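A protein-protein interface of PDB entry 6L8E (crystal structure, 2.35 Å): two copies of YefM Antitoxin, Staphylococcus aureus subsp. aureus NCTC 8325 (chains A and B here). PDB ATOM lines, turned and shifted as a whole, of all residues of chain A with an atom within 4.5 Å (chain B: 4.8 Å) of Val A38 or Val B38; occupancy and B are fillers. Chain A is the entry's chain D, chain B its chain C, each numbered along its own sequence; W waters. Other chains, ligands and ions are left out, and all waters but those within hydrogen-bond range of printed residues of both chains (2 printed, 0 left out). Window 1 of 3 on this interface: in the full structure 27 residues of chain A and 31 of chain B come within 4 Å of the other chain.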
ATOM      1  N   MET A   1     -19.560 -12.491 -17.227  1.00  0.00           N
ATOM      2  CA  MET A   1     -19.528 -11.100 -17.668  1.00  0.00           C
ATOM      3  C   MET A   1     -19.481 -11.005 -19.190  1.00  0.00           C
ATOM      4  O   MET A   1     -18.497 -11.392 -19.821  1.00  0.00           O
ATOM      5  CB  MET A   1     -18.325 -10.361 -17.066  1.00  0.00           C
ATOM      6  CG  MET A   1     -18.210  -8.899 -17.512  1.00  0.00           C
ATOM      7  SD  MET A   1     -19.557  -7.853 -16.919  1.00  0.00           S
ATOM      8  CE  MET A   1     -19.298  -7.915 -15.147  1.00  0.00           C
ATOM      9  N   MET A  26     -24.029 -10.120 -16.266  1.00  0.00           N
ATOM     10  CA  MET A  26     -23.906  -8.688 -16.462  1.00  0.00           C
ATOM     11  C   MET A  26     -23.209  -8.388 -17.778  1.00  0.00           C
ATOM     12  O   MET A  26     -22.604  -9.259 -18.408  1.00  0.00           O
ATOM     13  CB  MET A  26     -23.145  -8.038 -15.290  1.00  0.00           C
ATOM     14  CG  MET A  26     -23.743  -8.400 -13.933  1.00  0.00           C
ATOM     15  SD  MET A  26     -22.933  -7.799 -12.446  1.00  0.00           S
ATOM     16  CE  MET A  26     -23.766  -8.783 -11.203  1.00  0.00           C
ATOM     17  N   VAL A  27     -23.315  -7.127 -18.185  1.00  0.00           N
ATOM     18  CA  VAL A  27     -22.687  -6.628 -19.396  1.00  0.00           C
ATOM     19  C   VAL A  27     -21.868  -5.408 -19.023  1.00  0.00           C
ATOM     20  O   VAL A  27     -22.405  -4.441 -18.472  1.00  0.00           O
ATOM     21  CB  VAL A  27     -23.712  -6.266 -20.478  1.00  0.00           C
ATOM     22  CG1 VAL A  27     -22.994  -5.825 -21.740  1.00  0.00           C
ATOM     23  CG2 VAL A  27     -24.626  -7.441 -20.757  1.00  0.00           C
ATOM     24  N   THR A  28     -20.571  -5.463 -19.296  1.00  0.00           N
ATOM     25  CA  THR A  28     -19.756  -4.262 -19.377  1.00  0.00           C
ATOM     26  C   THR A  28     -19.793  -3.785 -20.818  1.00  0.00           C
ATOM     27  O   THR A  28     -19.377  -4.515 -21.725  1.00  0.00           O
ATOM     28  CB  THR A  28     -18.314  -4.528 -18.954  1.00  0.00           C
ATOM     29  OG1 THR A  28     -18.289  -5.107 -17.646  1.00  0.00           O
ATOM     30  CG2 THR A  28     -17.533  -3.228 -18.946  1.00  0.00           C
ATOM     31  N   VAL A  37     -19.708   1.356 -18.539  1.00  0.00           N
ATOM     32  CA  VAL A  37     -20.774   1.075 -17.587  1.00  0.00           C
ATOM     33  C   VAL A  37     -20.949  -0.434 -17.471  1.00  0.00           C
ATOM     34  O   VAL A  37     -20.502  -1.209 -18.319  1.00  0.00           O
ATOM     35  CB  VAL A  37     -22.115   1.741 -17.984  1.00  0.00           C
ATOM     36  CG1 VAL A  37     -21.942   3.247 -18.159  1.00  0.00           C
ATOM     37  CG2 VAL A  37     -22.692   1.106 -19.249  1.00  0.00           C
ATOM     38  N   VAL A  38     -21.610  -0.843 -16.392  1.00  0.00           N
ATOM     39  CA  VAL A  38     -21.998  -2.233 -16.179  1.00  0.00           C
ATOM     40  C   VAL A  38     -23.514  -2.285 -16.068  1.00  0.00           C
ATOM     41  O   VAL A  38     -24.119  -1.481 -15.349  1.00  0.00           O
ATOM     42  CB  VAL A  38     -21.335  -2.836 -14.927  1.00  0.00           C
ATOM     43  CG1 VAL A  38     -21.805  -4.266 -14.704  1.00  0.00           C
ATOM     44  CG2 VAL A  38     -19.821  -2.786 -15.057  1.00  0.00           C
ATOM     45  N   ILE A  39     -24.123  -3.224 -16.785  1.00  0.00           N
ATOM     46  CA  ILE A  39     -25.565  -3.423 -16.788  1.00  0.00           C
ATOM     47  C   ILE A  39     -25.855  -4.742 -16.093  1.00  0.00           C
ATOM     48  O   ILE A  39     -25.320  -5.788 -16.478  1.00  0.00           O
ATOM     49  CB  ILE A  39     -26.131  -3.419 -18.214  1.00  0.00           C
ATOM     50  CG1 ILE A  39     -25.693  -2.166 -18.966  1.00  0.00           C
ATOM     51  CG2 ILE A  39     -27.646  -3.506 -18.192  1.00  0.00           C
ATOM     52  CD1 ILE A  39     -26.145  -2.168 -20.405  1.00  0.00           C
ATOM     53  N   MET A  40     -26.702  -4.693 -15.071  1.00  0.00           N
ATOM     54  CA  MET A  40     -27.123  -5.877 -14.337  1.00  0.00           C
ATOM     55  C   MET A  40     -28.633  -5.835 -14.170  1.00  0.00           C
ATOM     56  O   MET A  40     -29.257  -4.782 -14.309  1.00  0.00           O
ATOM     57  CB  MET A  40     -26.458  -5.958 -12.958  1.00  0.00           C
ATOM     58  CG  MET A  40     -26.954  -4.900 -11.985  1.00  0.00           C
ATOM     59  SD  MET A  40     -25.884  -4.692 -10.554  1.00  0.00           S
ATOM     60  CE  MET A  40     -24.353  -4.188 -11.328  1.00  0.00           C
ATOM     61  N   SER A  41     -29.214  -6.990 -13.866  1.00  0.00           N
ATOM     62  CA  SER A  41     -30.649  -7.061 -13.636  1.00  0.00           C
ATOM     63  C   SER A  41     -31.007  -6.319 -12.355  1.00  0.00           C
ATOM     64  O   SER A  41     -30.228  -6.292 -11.395  1.00  0.00           O
ATOM     65  CB  SER A  41     -31.105  -8.520 -13.557  1.00  0.00           C
ATOM     66  OG  SER A  41     -30.880  -9.057 -12.264  1.00  0.00           O
ATOM     67  N   GLU A  42     -32.184  -5.686 -12.353  1.00  0.00           N
ATOM     68  CA  GLU A  42     -32.618  -4.964 -11.160  1.00  0.00           C
ATOM     69  C   GLU A  42     -32.758  -5.906  -9.974  1.00  0.00           C
ATOM     70  O   GLU A  42     -32.426  -5.544  -8.838  1.00  0.00           O
ATOM     71  CB  GLU A  42     -33.940  -4.241 -11.417  1.00  0.00           C
ATOM     72  CG  GLU A  42     -34.355  -3.319 -10.276  1.00  0.00           C
ATOM     73  CD  GLU A  42     -35.702  -2.660 -10.499  1.00  0.00           C
ATOM     74  OE1 GLU A  42     -36.514  -3.209 -11.273  1.00  0.00           O
ATOM     75  OE2 GLU A  42     -35.942  -1.587  -9.903  1.00  0.00           O
ATOM     76  N   TYR A  45     -29.393  -6.493  -8.568  1.00  0.00           N
ATOM     77  CA  TYR A  45     -28.965  -5.323  -7.807  1.00  0.00           C
ATOM     78  C   TYR A  45     -29.598  -5.314  -6.424  1.00  0.00           C
ATOM     79  O   TYR A  45     -28.926  -5.063  -5.416  1.00  0.00           O
ATOM     80  CB  TYR A  45     -29.308  -4.036  -8.547  1.00  0.00           C
ATOM     81  CG  TYR A  45     -28.938  -2.796  -7.760  1.00  0.00           C
ATOM     82  CD1 TYR A  45     -27.620  -2.359  -7.708  1.00  0.00           C
ATOM     83  CD2 TYR A  45     -29.896  -2.071  -7.060  1.00  0.00           C
ATOM     84  CE1 TYR A  45     -27.265  -1.232  -6.985  1.00  0.00           C
ATOM     85  CE2 TYR A  45     -29.555  -0.943  -6.337  1.00  0.00           C
ATOM     86  CZ  TYR A  45     -28.242  -0.528  -6.301  1.00  0.00           C
ATOM     87  OH  TYR A  45     -27.921   0.594  -5.574  1.00  0.00           O
ATOM     88  N   MET B   1     -31.180   7.264  -7.497  1.00  0.00           N
ATOM     89  CA  MET B   1     -31.418   6.395  -8.645  1.00  0.00           C
ATOM     90  C   MET B   1     -32.336   7.060  -9.667  1.00  0.00           C
ATOM     91  O   MET B   1     -33.530   7.239  -9.423  1.00  0.00           O
ATOM     92  CB  MET B   1     -32.021   5.058  -8.201  1.00  0.00           C
ATOM     93  CG  MET B   1     -32.220   4.062  -9.343  1.00  0.00           C
ATOM     94  SD  MET B   1     -30.706   3.208  -9.829  1.00  0.00           S
ATOM     95  CE  MET B   1     -30.383   2.224  -8.366  1.00  0.00           C
ATOM     96  N   VAL B  27     -28.727   4.504 -12.945  1.00  0.00           N
ATOM     97  CA  VAL B  27     -30.025   4.600 -13.599  1.00  0.00           C
ATOM     98  C   VAL B  27     -30.658   3.218 -13.634  1.00  0.00           C
ATOM     99  O   VAL B  27     -29.984   2.215 -13.900  1.00  0.00           O
ATOM    100  CB  VAL B  27     -29.934   5.212 -15.020  1.00  0.00           C
ATOM    101  CG1 VAL B  27     -29.085   6.475 -15.011  1.00  0.00           C
ATOM    102  CG2 VAL B  27     -29.411   4.209 -16.052  1.00  0.00           C
ATOM    103  N   THR B  28     -31.941   3.160 -13.304  1.00  0.00           N
ATOM    104  CA  THR B  28     -32.751   1.983 -13.563  1.00  0.00           C
ATOM    105  C   THR B  28     -33.477   2.187 -14.884  1.00  0.00           C
ATOM    106  O   THR B  28     -34.106   3.228 -15.099  1.00  0.00           O
ATOM    107  CB  THR B  28     -33.752   1.741 -12.432  1.00  0.00           C
ATOM    108  OG1 THR B  28     -33.051   1.457 -11.214  1.00  0.00           O
ATOM    109  CG2 THR B  28     -34.663   0.571 -12.770  1.00  0.00           C
ATOM    110  N   ASN B  36     -36.200  -5.376 -15.801  1.00  0.00           N
ATOM    111  CA  ASN B  36     -35.483  -4.118 -15.698  1.00  0.00           C
ATOM    112  C   ASN B  36     -34.001  -4.361 -15.432  1.00  0.00           C
ATOM    113  O   ASN B  36     -33.581  -5.444 -15.012  1.00  0.00           O
ATOM    114  CB  ASN B  36     -36.064  -3.254 -14.575  1.00  0.00           C
ATOM    115  CG  ASN B  36     -37.555  -3.027 -14.722  1.00  0.00           C
ATOM    116  OD1 ASN B  36     -38.114  -3.194 -15.805  1.00  0.00           O
ATOM    117  ND2 ASN B  36     -38.206  -2.642 -13.630  1.00  0.00           N
ATOM    118  N   VAL B  37     -33.208  -3.316 -15.674  1.00  0.00           N
ATOM    119  CA  VAL B  37     -31.779  -3.333 -15.411  1.00  0.00           C
ATOM    120  C   VAL B  37     -31.426  -2.061 -14.655  1.00  0.00           C
ATOM    121  O   VAL B  37     -32.156  -1.068 -14.691  1.00  0.00           O
ATOM    122  CB  VAL B  37     -30.942  -3.435 -16.705  1.00  0.00           C
ATOM    123  CG1 VAL B  37     -31.370  -4.633 -17.533  1.00  0.00           C
ATOM    124  CG2 VAL B  37     -31.069  -2.156 -17.520  1.00  0.00           C
ATOM    125  N   VAL B  38     -30.296  -2.104 -13.950  1.00  0.00           N
ATOM    126  CA  VAL B  38     -29.677  -0.896 -13.422  1.00  0.00           C
ATOM    127  C   VAL B  38     -28.299  -0.775 -14.054  1.00  0.00           C
ATOM    128  O   VAL B  38     -27.620  -1.773 -14.322  1.00  0.00           O
ATOM    129  CB  VAL B  38     -29.591  -0.860 -11.877  1.00  0.00           C
ATOM    130  CG1 VAL B  38     -30.527  -1.873 -11.268  1.00  0.00           C
ATOM    131  CG2 VAL B  38     -28.159  -1.050 -11.392  1.00  0.00           C
ATOM    132  N   ILE B  39     -27.912   0.464 -14.329  1.00  0.00           N
ATOM    133  CA  ILE B  39     -26.662   0.778 -15.001  1.00  0.00           C
ATOM    134  C   ILE B  39     -25.825   1.624 -14.056  1.00  0.00           C
ATOM    135  O   ILE B  39     -26.330   2.591 -13.475  1.00  0.00           O
ATOM    136  CB  ILE B  39     -26.907   1.512 -16.331  1.00  0.00           C
ATOM    137  CG1 ILE B  39     -27.805   0.668 -17.247  1.00  0.00           C
ATOM    138  CG2 ILE B  39     -25.593   1.869 -16.997  1.00  0.00           C
ATOM    139  CD1 ILE B  39     -28.143   1.335 -18.569  1.00  0.00           C
ATOM    140  N   MET B  40     -24.560   1.248 -13.883  1.00  0.00           N
ATOM    141  CA  MET B  40     -23.645   2.002 -13.039  1.00  0.00           C
ATOM    142  C   MET B  40     -22.301   2.072 -13.745  1.00  0.00           C
ATOM    143  O   MET B  40     -22.051   1.345 -14.706  1.00  0.00           O
ATOM    144  CB  MET B  40     -23.509   1.367 -11.650  1.00  0.00           C
ATOM    145  CG  MET B  40     -22.891  -0.021 -11.673  1.00  0.00           C
ATOM    146  SD  MET B  40     -22.925  -0.781 -10.045  1.00  0.00           S
ATOM    147  CE  MET B  40     -24.692  -0.865  -9.774  1.00  0.00           C
ATOM    148  N   SER B  41     -21.436   2.958 -13.264  1.00  0.00           N
ATOM    149  CA  SER B  41     -20.094   3.053 -13.821  1.00  0.00           C
ATOM    150  C   SER B  41     -19.304   1.782 -13.510  1.00  0.00           C
ATOM    151  O   SER B  41     -19.584   1.067 -12.544  1.00  0.00           O
ATOM    152  CB  SER B  41     -19.365   4.278 -13.270  1.00  0.00           C
ATOM    153  OG  SER B  41     -18.927   4.060 -11.940  1.00  0.00           O
ATOM    154  N   GLU B  42     -18.309   1.494 -14.356  1.00  0.00           N
ATOM    155  CA  GLU B  42     -17.469   0.326 -14.114  1.00  0.00           C
ATOM    156  C   GLU B  42     -16.709   0.456 -12.804  1.00  0.00           C
ATOM    157  O   GLU B  42     -16.422  -0.552 -12.145  1.00  0.00           O
ATOM    158  CB  GLU B  42     -16.491   0.112 -15.269  1.00  0.00           C
ATOM    159  CG  GLU B  42     -15.908  -1.297 -15.295  1.00  0.00           C
ATOM    160  CD  GLU B  42     -14.879  -1.503 -16.391  1.00  0.00           C
ATOM    161  OE1 GLU B  42     -14.173  -2.533 -16.368  1.00  0.00           O
ATOM    162  OE2 GLU B  42     -14.773  -0.630 -17.278  1.00  0.00           O
ATOM    163  N   TYR B  45     -19.121  -0.331 -10.025  1.00  0.00           N
ATOM    164  CA  TYR B  45     -19.341  -1.772 -10.009  1.00  0.00           C
ATOM    165  C   TYR B  45     -18.220  -2.491  -9.271  1.00  0.00           C
ATOM    166  O   TYR B  45     -18.474  -3.326  -8.393  1.00  0.00           O
ATOM    167  CB  TYR B  45     -19.463  -2.296 -11.433  1.00  0.00           C
ATOM    168  CG  TYR B  45     -19.465  -3.799 -11.510  1.00  0.00           C
ATOM    169  CD1 TYR B  45     -20.608  -4.517 -11.199  1.00  0.00           C
ATOM    170  CD2 TYR B  45     -18.325  -4.503 -11.884  1.00  0.00           C
ATOM    171  CE1 TYR B  45     -20.622  -5.886 -11.258  1.00  0.00           C
ATOM    172  CE2 TYR B  45     -18.329  -5.881 -11.950  1.00  0.00           C
ATOM    173  CZ  TYR B  45     -19.483  -6.568 -11.639  1.00  0.00           C
ATOM    174  OH  TYR B  45     -19.502  -7.943 -11.698  1.00  0.00           O
HETATM  175  O   HOH W   1     -34.153   0.132  -8.960  1.00  0.00           O
HETATM  176  O   HOH W   2     -34.645  -7.361 -12.504  1.00  0.00           O
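Met A1 touches Tyr B45 (CE to OH, 3.5 Å).
CB of Val A37 touches CG2 of Ile B39, 3.6 Å away.
Val A38 touches Val B38 (O to O, 3.7 Å).
Ile B39 touches Val A38 (CA to O, 3.4 Å).
O of Val B38 touches CA of Ile A39, at 3.6 Å.
Met A40 touches Val B37.
Met B40 touches Met A40 (CE to CE, 3.7 Å).
Thr B28 touches Glu A42.
Met B1 touches Tyr A45.
Val B38 touches Tyr A45.
The side-chain sulfur (SD) of Met B1 lies within hydrogen-bond range of the side-chain hydroxyl (OG1) of Thr B28 (3.2 Å).
N of Ile B39 lies within hydrogen-bond range of O of Val B27, 2.7 Å away.
The side-chain sulfur of Met A1 is in hydrogen-bond range of the side-chain hydroxyl of Thr A28 (3.1 Å).
The backbone NH (N) of Ile A39 is in hydrogen-bond range of the backbone carbonyl oxygen (O) of Val A27 (2.7 Å).
Printed residues of chain B within 4 Å of Val A38: Val B38, Ile B39, Met B40 and Tyr B45.
Val B38 touches just these residues of chain A: Val A38 (3.7 Å), Ile A39 (3.6 Å), Met A40 (2.9 Å), Glu A42 (3.7 Å) and Tyr A45 (3.7 Å).
Printed residues of chain B within 4 Å of Met A40: Val B37 (3.1 Å), Val B38 (2.9 Å), Met B40 (3.7 Å) and Tyr B45 (3.8 Å).
Of the printed residues of chain A, Ile B39 touches Val A37, Val A38 and Ile A39.
Thr A28 touches none of the printed residues of chain B.
Glu B42 touches none of the printed residues of chain A.
Val A38 touches its own counterpart, Val B38.
Val A38 touches Met B40, and with the chains exchanged Met A40 touches Val B38.
Met B40 touches its own counterpart, Met A40.
Met A40 touches Tyr B45, and with the chains exchanged Tyr A45 touches Met B40.
Of the 23 pairs that touch across the chains among the printed residues, 17 have their exchanged pair printed and touching as well.
Hydrophobic or aromatic side chains of chain A within 4 Å of the printed part of chain B: Met A1, Met A26, Val A37, Val A38, Ile A39, Met A40 and Tyr A45.
Printed residues of chain B that touch a printed residue of chain A: Met B1, Thr B28, Asn B36, Val B37, Val B38, Ile B39, Met B40 and Tyr B45.
Hydrophobic or aromatic side chains of chain B that line the printed part of chain A: Met B1, Val B37, Val B38, Ile B39, Met B40 and Tyr B45.
Among the printed residues, no Asp or Glu carboxylate lies within 4 Å of a Lys or Arg side-chain nitrogen of the other chain.
ND2 of Asn B36 lies within hydrogen-bond range of OE1 of Glu A42 (3.0 Å).
N of Val B38 sits at hydrogen-bond distance from O of Met A40, 2.9 Å away.
O of Met B40 sits at hydrogen-bond distance from N of Val A38, at 2.8 Å.
The side-chain hydroxyl (OH) of Tyr B45 sits close to the side-chain sulfur (SD) of Met A26 (3.5 Å).
Water W1 bridges OE2 of Glu A42 (2.7 Å) and OG1 of Thr B28 (2.8 Å).
Water W2 bridges N of Glu A42 (3.0 Å) and O of Asn B36 (3.3 Å).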
